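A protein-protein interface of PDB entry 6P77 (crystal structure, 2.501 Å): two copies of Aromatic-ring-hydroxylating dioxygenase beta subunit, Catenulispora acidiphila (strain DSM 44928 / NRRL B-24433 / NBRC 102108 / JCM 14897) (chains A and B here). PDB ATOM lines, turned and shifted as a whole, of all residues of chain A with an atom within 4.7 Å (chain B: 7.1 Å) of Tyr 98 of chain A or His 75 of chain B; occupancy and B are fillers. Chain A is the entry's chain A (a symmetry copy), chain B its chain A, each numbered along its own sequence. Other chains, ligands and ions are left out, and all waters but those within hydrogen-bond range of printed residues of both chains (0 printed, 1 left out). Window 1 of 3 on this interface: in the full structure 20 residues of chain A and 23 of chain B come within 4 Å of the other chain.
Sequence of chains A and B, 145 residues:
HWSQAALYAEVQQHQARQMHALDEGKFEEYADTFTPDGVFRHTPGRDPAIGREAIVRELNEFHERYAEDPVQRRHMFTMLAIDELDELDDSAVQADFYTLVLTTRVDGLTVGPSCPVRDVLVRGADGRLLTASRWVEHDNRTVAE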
ATOM      1  N   MET A  76      28.744   1.482  -4.933  1.00  0.00           N
ATOM      2  CA  MET A  76      28.625   0.535  -6.026  1.00  0.00           C
ATOM      3  C   MET A  76      27.272   0.661  -6.712  1.00  0.00           C
ATOM      4  O   MET A  76      26.240   0.434  -6.088  1.00  0.00           O
ATOM      5  CB  MET A  76      28.845  -0.857  -5.468  1.00  0.00           C
ATOM      6  CG  MET A  76      30.238  -0.932  -4.937  1.00  0.00           C
ATOM      7  SD  MET A  76      30.677  -2.621  -4.121  1.00  0.00           S
ATOM      8  CE  MET A  76      32.629  -2.526  -3.740  1.00  0.00           C
ATOM      9  N   PHE A  77      27.313   1.039  -7.997  1.00  0.00           N
ATOM     10  CA  PHE A  77      26.132   1.169  -8.833  1.00  0.00           C
ATOM     11  C   PHE A  77      25.870  -0.098  -9.637  1.00  0.00           C
ATOM     12  O   PHE A  77      26.777  -0.703 -10.141  1.00  0.00           O
ATOM     13  CB  PHE A  77      26.259   2.343  -9.798  1.00  0.00           C
ATOM     14  CG  PHE A  77      26.427   3.690  -9.144  1.00  0.00           C
ATOM     15  CD1 PHE A  77      26.455   3.860  -7.758  1.00  0.00           C
ATOM     16  CD2 PHE A  77      26.541   4.834  -9.945  1.00  0.00           C
ATOM     17  CE1 PHE A  77      26.581   5.143  -7.188  1.00  0.00           C
ATOM     18  CE2 PHE A  77      26.686   6.095  -9.381  1.00  0.00           C
ATOM     19  CZ  PHE A  77      26.719   6.241  -7.987  1.00  0.00           C
ATOM     20  N   THR A  78      24.601  -0.489  -9.720  1.00  0.00           N
ATOM     21  CA  THR A  78      24.145  -1.561 -10.571  1.00  0.00           C
ATOM     22  C   THR A  78      22.766  -1.177 -11.117  1.00  0.00           C
ATOM     23  O   THR A  78      22.121  -0.252 -10.636  1.00  0.00           O
ATOM     24  CB  THR A  78      24.098  -2.915  -9.794  1.00  0.00           C
ATOM     25  OG1 THR A  78      23.095  -2.858  -8.753  1.00  0.00           O
ATOM     26  CG2 THR A  78      25.496  -3.264  -9.162  1.00  0.00           C
ATOM     27  N   MET A  79      22.334  -1.903 -12.149  1.00  0.00           N
ATOM     28  CA  MET A  79      20.974  -1.875 -12.668  1.00  0.00           C
ATOM     29  C   MET A  79      20.695  -0.504 -13.285  1.00  0.00           C
ATOM     30  O   MET A  79      19.692   0.133 -12.980  1.00  0.00           O
ATOM     31  CB  MET A  79      19.997  -2.271 -11.559  1.00  0.00           C
ATOM     32  CG  MET A  79      20.355  -3.571 -10.868  1.00  0.00           C
ATOM     33  SD  MET A  79      20.578  -5.157 -12.027  1.00  0.00           S
ATOM     34  CE  MET A  79      22.360  -4.892 -12.760  1.00  0.00           C
ATOM     35  N   PHE A  97      18.961   3.806 -11.512  1.00  0.00           N
ATOM     36  CA  PHE A  97      19.918   2.817 -11.064  1.00  0.00           C
ATOM     37  C   PHE A  97      19.881   2.606  -9.560  1.00  0.00           C
ATOM     38  O   PHE A  97      19.192   3.308  -8.835  1.00  0.00           O
ATOM     39  CB  PHE A  97      21.333   3.172 -11.534  1.00  0.00           C
ATOM     40  CG  PHE A  97      21.869   4.452 -10.973  1.00  0.00           C
ATOM     41  CD1 PHE A  97      21.575   5.677 -11.571  1.00  0.00           C
ATOM     42  CD2 PHE A  97      22.710   4.438  -9.873  1.00  0.00           C
ATOM     43  CE1 PHE A  97      22.080   6.849 -11.044  1.00  0.00           C
ATOM     44  CE2 PHE A  97      23.220   5.615  -9.348  1.00  0.00           C
ATOM     45  CZ  PHE A  97      22.902   6.817  -9.937  1.00  0.00           C
ATOM     46  N   TYR A  98      20.605   1.573  -9.125  1.00  0.00           N
ATOM     47  CA  TYR A  98      20.731   1.193  -7.741  1.00  0.00           C
ATOM     48  C   TYR A  98      22.138   1.514  -7.234  1.00  0.00           C
ATOM     49  O   TYR A  98      23.113   1.373  -7.956  1.00  0.00           O
ATOM     50  CB  TYR A  98      20.458  -0.299  -7.572  1.00  0.00           C
ATOM     51  CG  TYR A  98      19.038  -0.811  -7.822  1.00  0.00           C
ATOM     52  CD1 TYR A  98      17.918   0.021  -7.841  1.00  0.00           C
ATOM     53  CD2 TYR A  98      18.822  -2.166  -7.980  1.00  0.00           C
ATOM     54  CE1 TYR A  98      16.639  -0.495  -8.055  1.00  0.00           C
ATOM     55  CE2 TYR A  98      17.559  -2.687  -8.156  1.00  0.00           C
ATOM     56  CZ  TYR A  98      16.483  -1.851  -8.212  1.00  0.00           C
ATOM     57  OH  TYR A  98      15.278  -2.464  -8.376  1.00  0.00           O
ATOM     58  N   THR A  99      22.214   1.967  -5.983  1.00  0.00           N
ATOM     59  CA  THR A  99      23.462   2.219  -5.294  1.00  0.00           C
ATOM     60  C   THR A  99      23.477   1.354  -4.046  1.00  0.00           C
ATOM     61  O   THR A  99      22.477   1.232  -3.358  1.00  0.00           O
ATOM     62  CB  THR A  99      23.613   3.701  -4.862  1.00  0.00           C
ATOM     63  OG1 THR A  99      23.570   4.558  -6.013  1.00  0.00           O
ATOM     64  CG2 THR A  99      24.972   3.910  -4.181  1.00  0.00           C
ATOM     65  N   LEU A 100      24.626   0.718  -3.802  1.00  0.00           N
ATOM     66  CA  LEU A 100      24.933   0.031  -2.573  1.00  0.00           C
ATOM     67  C   LEU A 100      26.154   0.725  -1.928  1.00  0.00           C
ATOM     68  O   LEU A 100      27.203   0.823  -2.536  1.00  0.00           O
ATOM     69  CB  LEU A 100      25.229  -1.424  -2.836  1.00  0.00           C
ATOM     70  CG  LEU A 100      25.385  -2.243  -1.545  1.00  0.00           C
ATOM     71  CD1 LEU A 100      24.107  -2.183  -0.726  1.00  0.00           C
ATOM     72  CD2 LEU A 100      25.823  -3.679  -1.844  1.00  0.00           C
ATOM     73  N   CYS A 115      20.049   2.316  -2.153  1.00  0.00           N
ATOM     74  CA  CYS A 115      19.437   3.550  -2.586  1.00  0.00           C
ATOM     75  C   CYS A 115      19.093   3.543  -4.075  1.00  0.00           C
ATOM     76  O   CYS A 115      19.973   3.566  -4.942  1.00  0.00           O
ATOM     77  CB  CYS A 115      20.421   4.696  -2.296  1.00  0.00           C
ATOM     78  SG  CYS A 115      20.941   4.858  -0.562  1.00  0.00           S
ATOM     79  N   PRO A 116      17.799   3.515  -4.442  1.00  0.00           N
ATOM     80  CA  PRO A 116      17.422   3.818  -5.820  1.00  0.00           C
ATOM     81  C   PRO A 116      17.752   5.282  -6.083  1.00  0.00           C
ATOM     82  O   PRO A 116      17.488   6.129  -5.224  1.00  0.00           O
ATOM     83  CB  PRO A 116      15.904   3.587  -5.859  1.00  0.00           C
ATOM     84  CG  PRO A 116      15.456   3.432  -4.469  1.00  0.00           C
ATOM     85  CD  PRO A 116      16.659   3.234  -3.561  1.00  0.00           C
ATOM     86  N   GLN B  15      17.892  -6.201 -18.425  1.00  0.00           N
ATOM     87  CA  GLN B  15      17.975  -6.795 -17.107  1.00  0.00           C
ATOM     88  C   GLN B  15      17.651  -5.779 -16.007  1.00  0.00           C
ATOM     89  O   GLN B  15      16.863  -6.049 -15.088  1.00  0.00           O
ATOM     90  CB  GLN B  15      19.351  -7.454 -16.916  1.00  0.00           C
ATOM     91  CG  GLN B  15      19.476  -8.735 -17.710  1.00  0.00           C
ATOM     92  CD  GLN B  15      20.787  -9.453 -17.503  1.00  0.00           C
ATOM     93  OE1 GLN B  15      21.802  -8.811 -17.314  1.00  0.00           O
ATOM     94  NE2 GLN B  15      20.780 -10.813 -17.600  1.00  0.00           N
ATOM     95  N   ALA B  16      18.215  -4.579 -16.127  1.00  0.00           N
ATOM     96  CA  ALA B  16      17.941  -3.511 -15.168  1.00  0.00           C
ATOM     97  C   ALA B  16      16.437  -3.229 -15.077  1.00  0.00           C
ATOM     98  O   ALA B  16      15.888  -3.211 -13.993  1.00  0.00           O
ATOM     99  CB  ALA B  16      18.702  -2.235 -15.544  1.00  0.00           C
ATOM    100  N   GLN B  18      13.891  -5.034 -15.975  1.00  0.00           N
ATOM    101  CA  GLN B  18      13.240  -6.192 -15.388  1.00  0.00           C
ATOM    102  C   GLN B  18      13.241  -6.101 -13.859  1.00  0.00           C
ATOM    103  O   GLN B  18      12.210  -6.328 -13.219  1.00  0.00           O
ATOM    104  CB  GLN B  18      13.922  -7.487 -15.776  1.00  0.00           C
ATOM    105  CG  GLN B  18      13.606  -8.016 -17.134  1.00  0.00           C
ATOM    106  CD  GLN B  18      14.267  -9.376 -17.373  1.00  0.00           C
ATOM    107  OE1 GLN B  18      15.442  -9.574 -17.058  1.00  0.00           O
ATOM    108  NE2 GLN B  18      13.506 -10.313 -17.949  1.00  0.00           N
ATOM    109  N   MET B  19      14.407  -5.807 -13.277  1.00  0.00           N
ATOM    110  CA  MET B  19      14.529  -5.810 -11.828  1.00  0.00           C
ATOM    111  C   MET B  19      13.872  -4.567 -11.237  1.00  0.00           C
ATOM    112  O   MET B  19      13.295  -4.645 -10.161  1.00  0.00           O
ATOM    113  CB  MET B  19      15.986  -5.909 -11.358  1.00  0.00           C
ATOM    114  CG  MET B  19      16.676  -7.243 -11.612  1.00  0.00           C
ATOM    115  SD  MET B  19      15.573  -8.820 -11.121  1.00  0.00           S
ATOM    116  CE  MET B  19      14.565  -9.340 -12.621  1.00  0.00           C
ATOM    117  N   HIS B  20      13.935  -3.426 -11.929  1.00  0.00           N
ATOM    118  CA  HIS B  20      13.211  -2.255 -11.457  1.00  0.00           C
ATOM    119  C   HIS B  20      11.710  -2.572 -11.287  1.00  0.00           C
ATOM    120  O   HIS B  20      11.081  -2.112 -10.319  1.00  0.00           O
ATOM    121  CB  HIS B  20      13.415  -1.014 -12.354  1.00  0.00           C
ATOM    122  CG  HIS B  20      14.841  -0.561 -12.440  1.00  0.00           C
ATOM    123  ND1 HIS B  20      15.273   0.381 -13.336  1.00  0.00           N
ATOM    124  CD2 HIS B  20      15.934  -0.912 -11.722  1.00  0.00           C
ATOM    125  CE1 HIS B  20      16.566   0.592 -13.182  1.00  0.00           C
ATOM    126  NE2 HIS B  20      16.998  -0.197 -12.216  1.00  0.00           N
ATOM    127  N   ALA B  21      11.151  -3.356 -12.222  1.00  0.00           N
ATOM    128  CA  ALA B  21       9.745  -3.719 -12.175  1.00  0.00           C
ATOM    129  C   ALA B  21       9.489  -4.679 -10.995  1.00  0.00           C
ATOM    130  O   ALA B  21       8.613  -4.431 -10.148  1.00  0.00           O
ATOM    131  CB  ALA B  21       9.319  -4.336 -13.509  1.00  0.00           C
ATOM    132  N   LEU B  22      10.288  -5.755 -10.945  1.00  0.00           N
ATOM    133  CA  LEU B  22      10.188  -6.812  -9.935  1.00  0.00           C
ATOM    134  C   LEU B  22      10.307  -6.289  -8.501  1.00  0.00           C
ATOM    135  O   LEU B  22       9.457  -6.562  -7.651  1.00  0.00           O
ATOM    136  CB  LEU B  22      11.271  -7.891 -10.157  1.00  0.00           C
ATOM    137  CG  LEU B  22      11.126  -9.080  -9.175  1.00  0.00           C
ATOM    138  CD1 LEU B  22       9.787  -9.762  -9.360  1.00  0.00           C
ATOM    139  CD2 LEU B  22      12.227 -10.111  -9.319  1.00  0.00           C
ATOM    140  N   ASP B  23      11.371  -5.525  -8.252  1.00  0.00           N
ATOM    141  CA  ASP B  23      11.695  -5.010  -6.952  1.00  0.00           C
ATOM    142  C   ASP B  23      10.610  -4.070  -6.450  1.00  0.00           C
ATOM    143  O   ASP B  23      10.419  -3.936  -5.254  1.00  0.00           O
ATOM    144  CB  ASP B  23      13.067  -4.317  -6.978  1.00  0.00           C
ATOM    145  CG  ASP B  23      14.245  -5.308  -7.142  1.00  0.00           C
ATOM    146  OD1 ASP B  23      14.070  -6.523  -6.904  1.00  0.00           O
ATOM    147  OD2 ASP B  23      15.364  -4.866  -7.533  1.00  0.00           O
ATOM    148  N   GLU B  24       9.892  -3.419  -7.365  1.00  0.00           N
ATOM    149  CA  GLU B  24       8.840  -2.484  -6.992  1.00  0.00           C
ATOM    150  C   GLU B  24       7.474  -3.149  -6.979  1.00  0.00           C
ATOM    151  O   GLU B  24       6.455  -2.469  -6.891  1.00  0.00           O
ATOM    152  CB  GLU B  24       8.838  -1.298  -7.949  1.00  0.00           C
ATOM    153  CG  GLU B  24      10.148  -0.496  -7.957  1.00  0.00           C
ATOM    154  CD  GLU B  24      10.364   0.289  -6.695  1.00  0.00           C
ATOM    155  OE1 GLU B  24       9.388   0.692  -6.073  1.00  0.00           O
ATOM    156  OE2 GLU B  24      11.513   0.479  -6.282  1.00  0.00           O
ATOM    157  N   GLN B  72      11.633  -4.275   1.414  1.00  0.00           N
ATOM    158  CA  GLN B  72      12.099  -3.829   0.118  1.00  0.00           C
ATOM    159  C   GLN B  72      13.309  -4.662  -0.298  1.00  0.00           C
ATOM    160  O   GLN B  72      14.360  -4.640   0.355  1.00  0.00           O
ATOM    161  CB  GLN B  72      12.487  -2.344   0.162  1.00  0.00           C
ATOM    162  CG  GLN B  72      13.015  -1.819  -1.169  1.00  0.00           C
ATOM    163  CD  GLN B  72      11.966  -1.890  -2.236  1.00  0.00           C
ATOM    164  OE1 GLN B  72      10.907  -1.292  -2.059  1.00  0.00           O
ATOM    165  NE2 GLN B  72      12.218  -2.653  -3.333  1.00  0.00           N
ATOM    166  N   ARG B  73      13.149  -5.385  -1.407  1.00  0.00           N
ATOM    167  CA  ARG B  73      14.167  -6.219  -1.985  1.00  0.00           C
ATOM    168  C   ARG B  73      14.799  -5.457  -3.165  1.00  0.00           C
ATOM    169  O   ARG B  73      14.141  -4.641  -3.822  1.00  0.00           O
ATOM    170  CB  ARG B  73      13.542  -7.580  -2.366  1.00  0.00           C
ATOM    171  CG  ARG B  73      14.532  -8.662  -2.841  1.00  0.00           C
ATOM    172  CD  ARG B  73      14.139 -10.131  -2.579  1.00  0.00           C
ATOM    173  NE  ARG B  73      13.051 -10.383  -1.611  1.00  0.00           N
ATOM    174  CZ  ARG B  73      13.118 -11.152  -0.504  1.00  0.00           C
ATOM    175  NH1 ARG B  73      14.252 -11.779  -0.164  1.00  0.00           N
ATOM    176  NH2 ARG B  73      12.031 -11.299   0.287  1.00  0.00           N
ATOM    177  N   ARG B  74      16.111  -5.642  -3.347  1.00  0.00           N
ATOM    178  CA  ARG B  74      16.851  -5.154  -4.515  1.00  0.00           C
ATOM    179  C   ARG B  74      17.699  -6.307  -5.042  1.00  0.00           C
ATOM    180  O   ARG B  74      18.362  -7.001  -4.266  1.00  0.00           O
ATOM    181  CB  ARG B  74      17.764  -3.974  -4.187  1.00  0.00           C
ATOM    182  CG  ARG B  74      17.081  -2.722  -3.711  1.00  0.00           C
ATOM    183  CD  ARG B  74      16.308  -2.016  -4.807  1.00  0.00           C
ATOM    184  NE  ARG B  74      15.422  -1.000  -4.225  1.00  0.00           N
ATOM    185  CZ  ARG B  74      14.332  -0.484  -4.790  1.00  0.00           C
ATOM    186  NH1 ARG B  74      13.929  -0.860  -5.985  1.00  0.00           N
ATOM    187  NH2 ARG B  74      13.645   0.434  -4.151  1.00  0.00           N
ATOM    188  N   HIS B  75      17.653  -6.537  -6.359  1.00  0.00           N
ATOM    189  CA  HIS B  75      18.544  -7.493  -7.005  1.00  0.00           C
ATOM    190  C   HIS B  75      19.607  -6.740  -7.794  1.00  0.00           C
ATOM    191  O   HIS B  75      19.283  -5.900  -8.633  1.00  0.00           O
ATOM    192  CB  HIS B  75      17.797  -8.373  -7.970  1.00  0.00           C
ATOM    193  CG  HIS B  75      16.747  -9.225  -7.341  1.00  0.00           C
ATOM    194  ND1 HIS B  75      15.527  -8.716  -6.940  1.00  0.00           N
ATOM    195  CD2 HIS B  75      16.700 -10.556  -7.111  1.00  0.00           C
ATOM    196  CE1 HIS B  75      14.785  -9.697  -6.462  1.00  0.00           C
ATOM    197  NE2 HIS B  75      15.467 -10.824  -6.567  1.00  0.00           N
ATOM    198  N   MET B  76      20.868  -7.084  -7.517  1.00  0.00           N
ATOM    199  CA  MET B  76      22.024  -6.477  -8.151  1.00  0.00           C
ATOM    200  C   MET B  76      22.791  -7.497  -8.980  1.00  0.00           C
ATOM    201  O   MET B  76      23.302  -8.472  -8.438  1.00  0.00           O
ATOM    202  CB  MET B  76      22.889  -5.868  -7.066  1.00  0.00           C
ATOM    203  CG  MET B  76      22.106  -4.789  -6.393  1.00  0.00           C
ATOM    204  SD  MET B  76      23.031  -3.943  -4.931  1.00  0.00           S
ATOM    205  CE  MET B  76      21.876  -2.411  -4.399  1.00  0.00           C
ATOM    206  N   PHE B  77      22.839  -7.247 -10.295  1.00  0.00           N
ATOM    207  CA  PHE B  77      23.563  -8.077 -11.243  1.00  0.00           C
ATOM    208  C   PHE B  77      24.964  -7.543 -11.503  1.00  0.00           C
ATOM    209  O   PHE B  77      25.160  -6.363 -11.619  1.00  0.00           O
ATOM    210  CB  PHE B  77      22.823  -8.179 -12.573  1.00  0.00           C
ATOM    211  CG  PHE B  77      21.446  -8.785 -12.492  1.00  0.00           C
ATOM    212  CD1 PHE B  77      20.886  -9.232 -11.294  1.00  0.00           C
ATOM    213  CD2 PHE B  77      20.690  -8.931 -13.662  1.00  0.00           C
ATOM    214  CE1 PHE B  77      19.605  -9.823 -11.269  1.00  0.00           C
ATOM    215  CE2 PHE B  77      19.420  -9.495 -13.631  1.00  0.00           C
ATOM    216  CZ  PHE B  77      18.874  -9.930 -12.416  1.00  0.00           C
ATOM    217  N   THR B  99      24.007 -12.611  -9.409  1.00  0.00           N
ATOM    218  CA  THR B  99      22.982 -11.840  -8.739  1.00  0.00           C
ATOM    219  C   THR B  99      23.316 -11.827  -7.258  1.00  0.00           C
ATOM    220  O   THR B  99      23.707 -12.836  -6.696  1.00  0.00           O
ATOM    221  CB  THR B  99      21.568 -12.452  -8.916  1.00  0.00           C
ATOM    222  OG1 THR B  99      21.227 -12.514 -10.309  1.00  0.00           O
ATOM    223  CG2 THR B  99      20.525 -11.564  -8.223  1.00  0.00           C
ATOM    224  N   LEU B 100      23.196 -10.642  -6.652  1.00  0.00           N
ATOM    225  CA  LEU B 100      23.245 -10.446  -5.226  1.00  0.00           C
ATOM    226  C   LEU B 100      21.883  -9.870  -4.774  1.00  0.00           C
ATOM    227  O   LEU B 100      21.464  -8.830  -5.248  1.00  0.00           O
ATOM    228  CB  LEU B 100      24.366  -9.508  -4.855  1.00  0.00           C
ATOM    229  CG  LEU B 100      24.579  -9.406  -3.336  1.00  0.00           C
ATOM    230  CD1 LEU B 100      24.920 -10.769  -2.760  1.00  0.00           C
ATOM    231  CD2 LEU B 100      25.625  -8.344  -2.990  1.00  0.00           C
ATOM    232  N   VAL B 101      21.198 -10.588  -3.878  1.00  0.00           N
ATOM    233  CA  VAL B 101      19.952 -10.135  -3.261  1.00  0.00           C
ATOM    234  C   VAL B 101      20.201  -9.295  -2.021  1.00  0.00           C
ATOM    235  O   VAL B 101      21.006  -9.671  -1.175  1.00  0.00           O
ATOM    236  CB  VAL B 101      19.074 -11.340  -2.860  1.00  0.00           C
ATOM    237  CG1 VAL B 101      17.768 -10.874  -2.245  1.00  0.00           C
ATOM    238  CG2 VAL B 101      18.786 -12.177  -4.083  1.00  0.00           C
ATOM    239  N   LEU B 102      19.515  -8.144  -1.930  1.00  0.00           N
ATOM    240  CA  LEU B 102      19.502  -7.278  -0.749  1.00  0.00           C
ATOM    241  C   LEU B 102      18.070  -7.112  -0.291  1.00  0.00           C
ATOM    242  O   LEU B 102      17.211  -6.835  -1.090  1.00  0.00           O
ATOM    243  CB  LEU B 102      20.055  -5.906  -1.054  1.00  0.00           C
ATOM    244  CG  LEU B 102      21.485  -5.867  -1.619  1.00  0.00           C
ATOM    245  CD1 LEU B 102      21.812  -4.434  -1.907  1.00  0.00           C
ATOM    246  CD2 LEU B 102      22.538  -6.422  -0.660  1.00  0.00           C
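Hydrophobic or aromatic side chains of chain B that line the printed part of chain A: Ala 16, His 20, Met 76, Phe 77 and Leu 102. Hydrophobic or aromatic side chains of chain A within 4 Å of the printed part of chain B: Met 79, Tyr 98, Leu 100 and Pro 116. Among the printed residues, no Asp or Glu carboxylate lies within 4 Å of a Lys or Arg side-chain nitrogen of the other chain.
Thr 99 of chain A touches Met 76 of chain B, but with the chains exchanged Met 76 of chain A does not touch Thr 99 of chain B (12.2 Å). Leu 100 of chain A touches Met 76 of chain B, but with the chains exchanged Met 76 of chain A does not touch Leu 100 of chain B (7.7 Å). Positions printed for both chains: 76, 77, 99 and 100.
Met 76 of chain B touches Thr 78 of chain A (CG to OG1, 3.2 Å). Thr 78 of chain A touches Phe 77 of chain B. Met 79 of chain A touches Ala 16 of chain B. His 20 of chain B touches Tyr 98 of chain A (CD2 to CZ, 3.7 Å). CE2 of Tyr 98 of chain A touches O of His 75 of chain B (3.7 Å). CE of Met 76 of chain B touches O of Thr 99 of chain A (3.8 Å). CB of Leu 100 of chain A touches CE of Met 76 of chain B, 3.8 Å away. Leu 100 of chain A touches Leu 102 of chain B. Arg 74 of chain B touches Pro 116 of chain A (NH2 to CG, 3.5 Å).
SD of Met 79 of chain A sits close to N of Phe 77 of chain B (3.5 Å). OH of Tyr 98 of chain A sits at hydrogen-bond distance from OD2 of Asp 23 of chain B (2.5 Å). A ring nitrogen (NE2) of His 20 of chain B lies within hydrogen-bond range of the backbone carbonyl oxygen of Met 79 of chain A (2.8 Å). O of Met 19 of chain B is in hydrogen-bond range of OH of Tyr 98 of chain A, 3.4 Å away. The guanidinium group of Arg 74 of chain B is in hydrogen-bond range of the side-chain hydroxyl of Tyr 98 of chain A. The side-chain sulfur (SD) of Met 79 of chain A sits close to the backbone carbonyl oxygen (O) of His 75 of chain B (3.7 Å).
The side-chain amide nitrogen (NE2) of Gln 72 of chain B lies within hydrogen-bond range of the backbone carbonyl oxygen (O) of Asp 23 of chain B, at 2.9 Å. N of Leu 100 of chain A sits at hydrogen-bond distance from O of Met 76 of chain A. The backbone carbonyl oxygen of Met 76 of chain B sits at hydrogen-bond distance from the backbone NH of Leu 100 of chain B. The backbone NH of Arg 74 of chain B lies within hydrogen-bond range of the backbone carbonyl oxygen of Leu 102 of chain B, 2.8 Å away. NH1 of Arg 74 of chain B lies within salt-bridge range of OE2 of Glu 24 of chain B (2.8 Å). The side-chain carboxylate (OD1) of Asp 23 of chain B sits at hydrogen-bond distance from a ring nitrogen (ND1) of His 75 of chain B (2.6 Å).
Printed residues of chain B within 4 Å of Met 79 of chain A: Ala 16 (3.5 Å), His 20 (2.8 Å), His 75 (3.4 Å) and Phe 77 (3.3 Å). Tyr 98 of chain A touches five residues of chain B. Printed residues of chain A within 4 Å of Ala 16 of chain B: Met 79 (3.5 Å). Gln 18 of chain B touches none of the printed residues of chain A. Ala 21 of chain B touches none of the printed residues of chain A. Of the printed residues of chain A, Arg 74 of chain B touches Tyr 98 (3.2 Å) and Pro 116 (3.5 Å). His 75 of chain B touches two residues of chain A. Of the printed residues of chain A, Leu 102 of chain B touches Leu 100. The nearest printed residue of chain A that does not touch His 75 of chain B is Thr 78 of chain A (4.9 Å).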
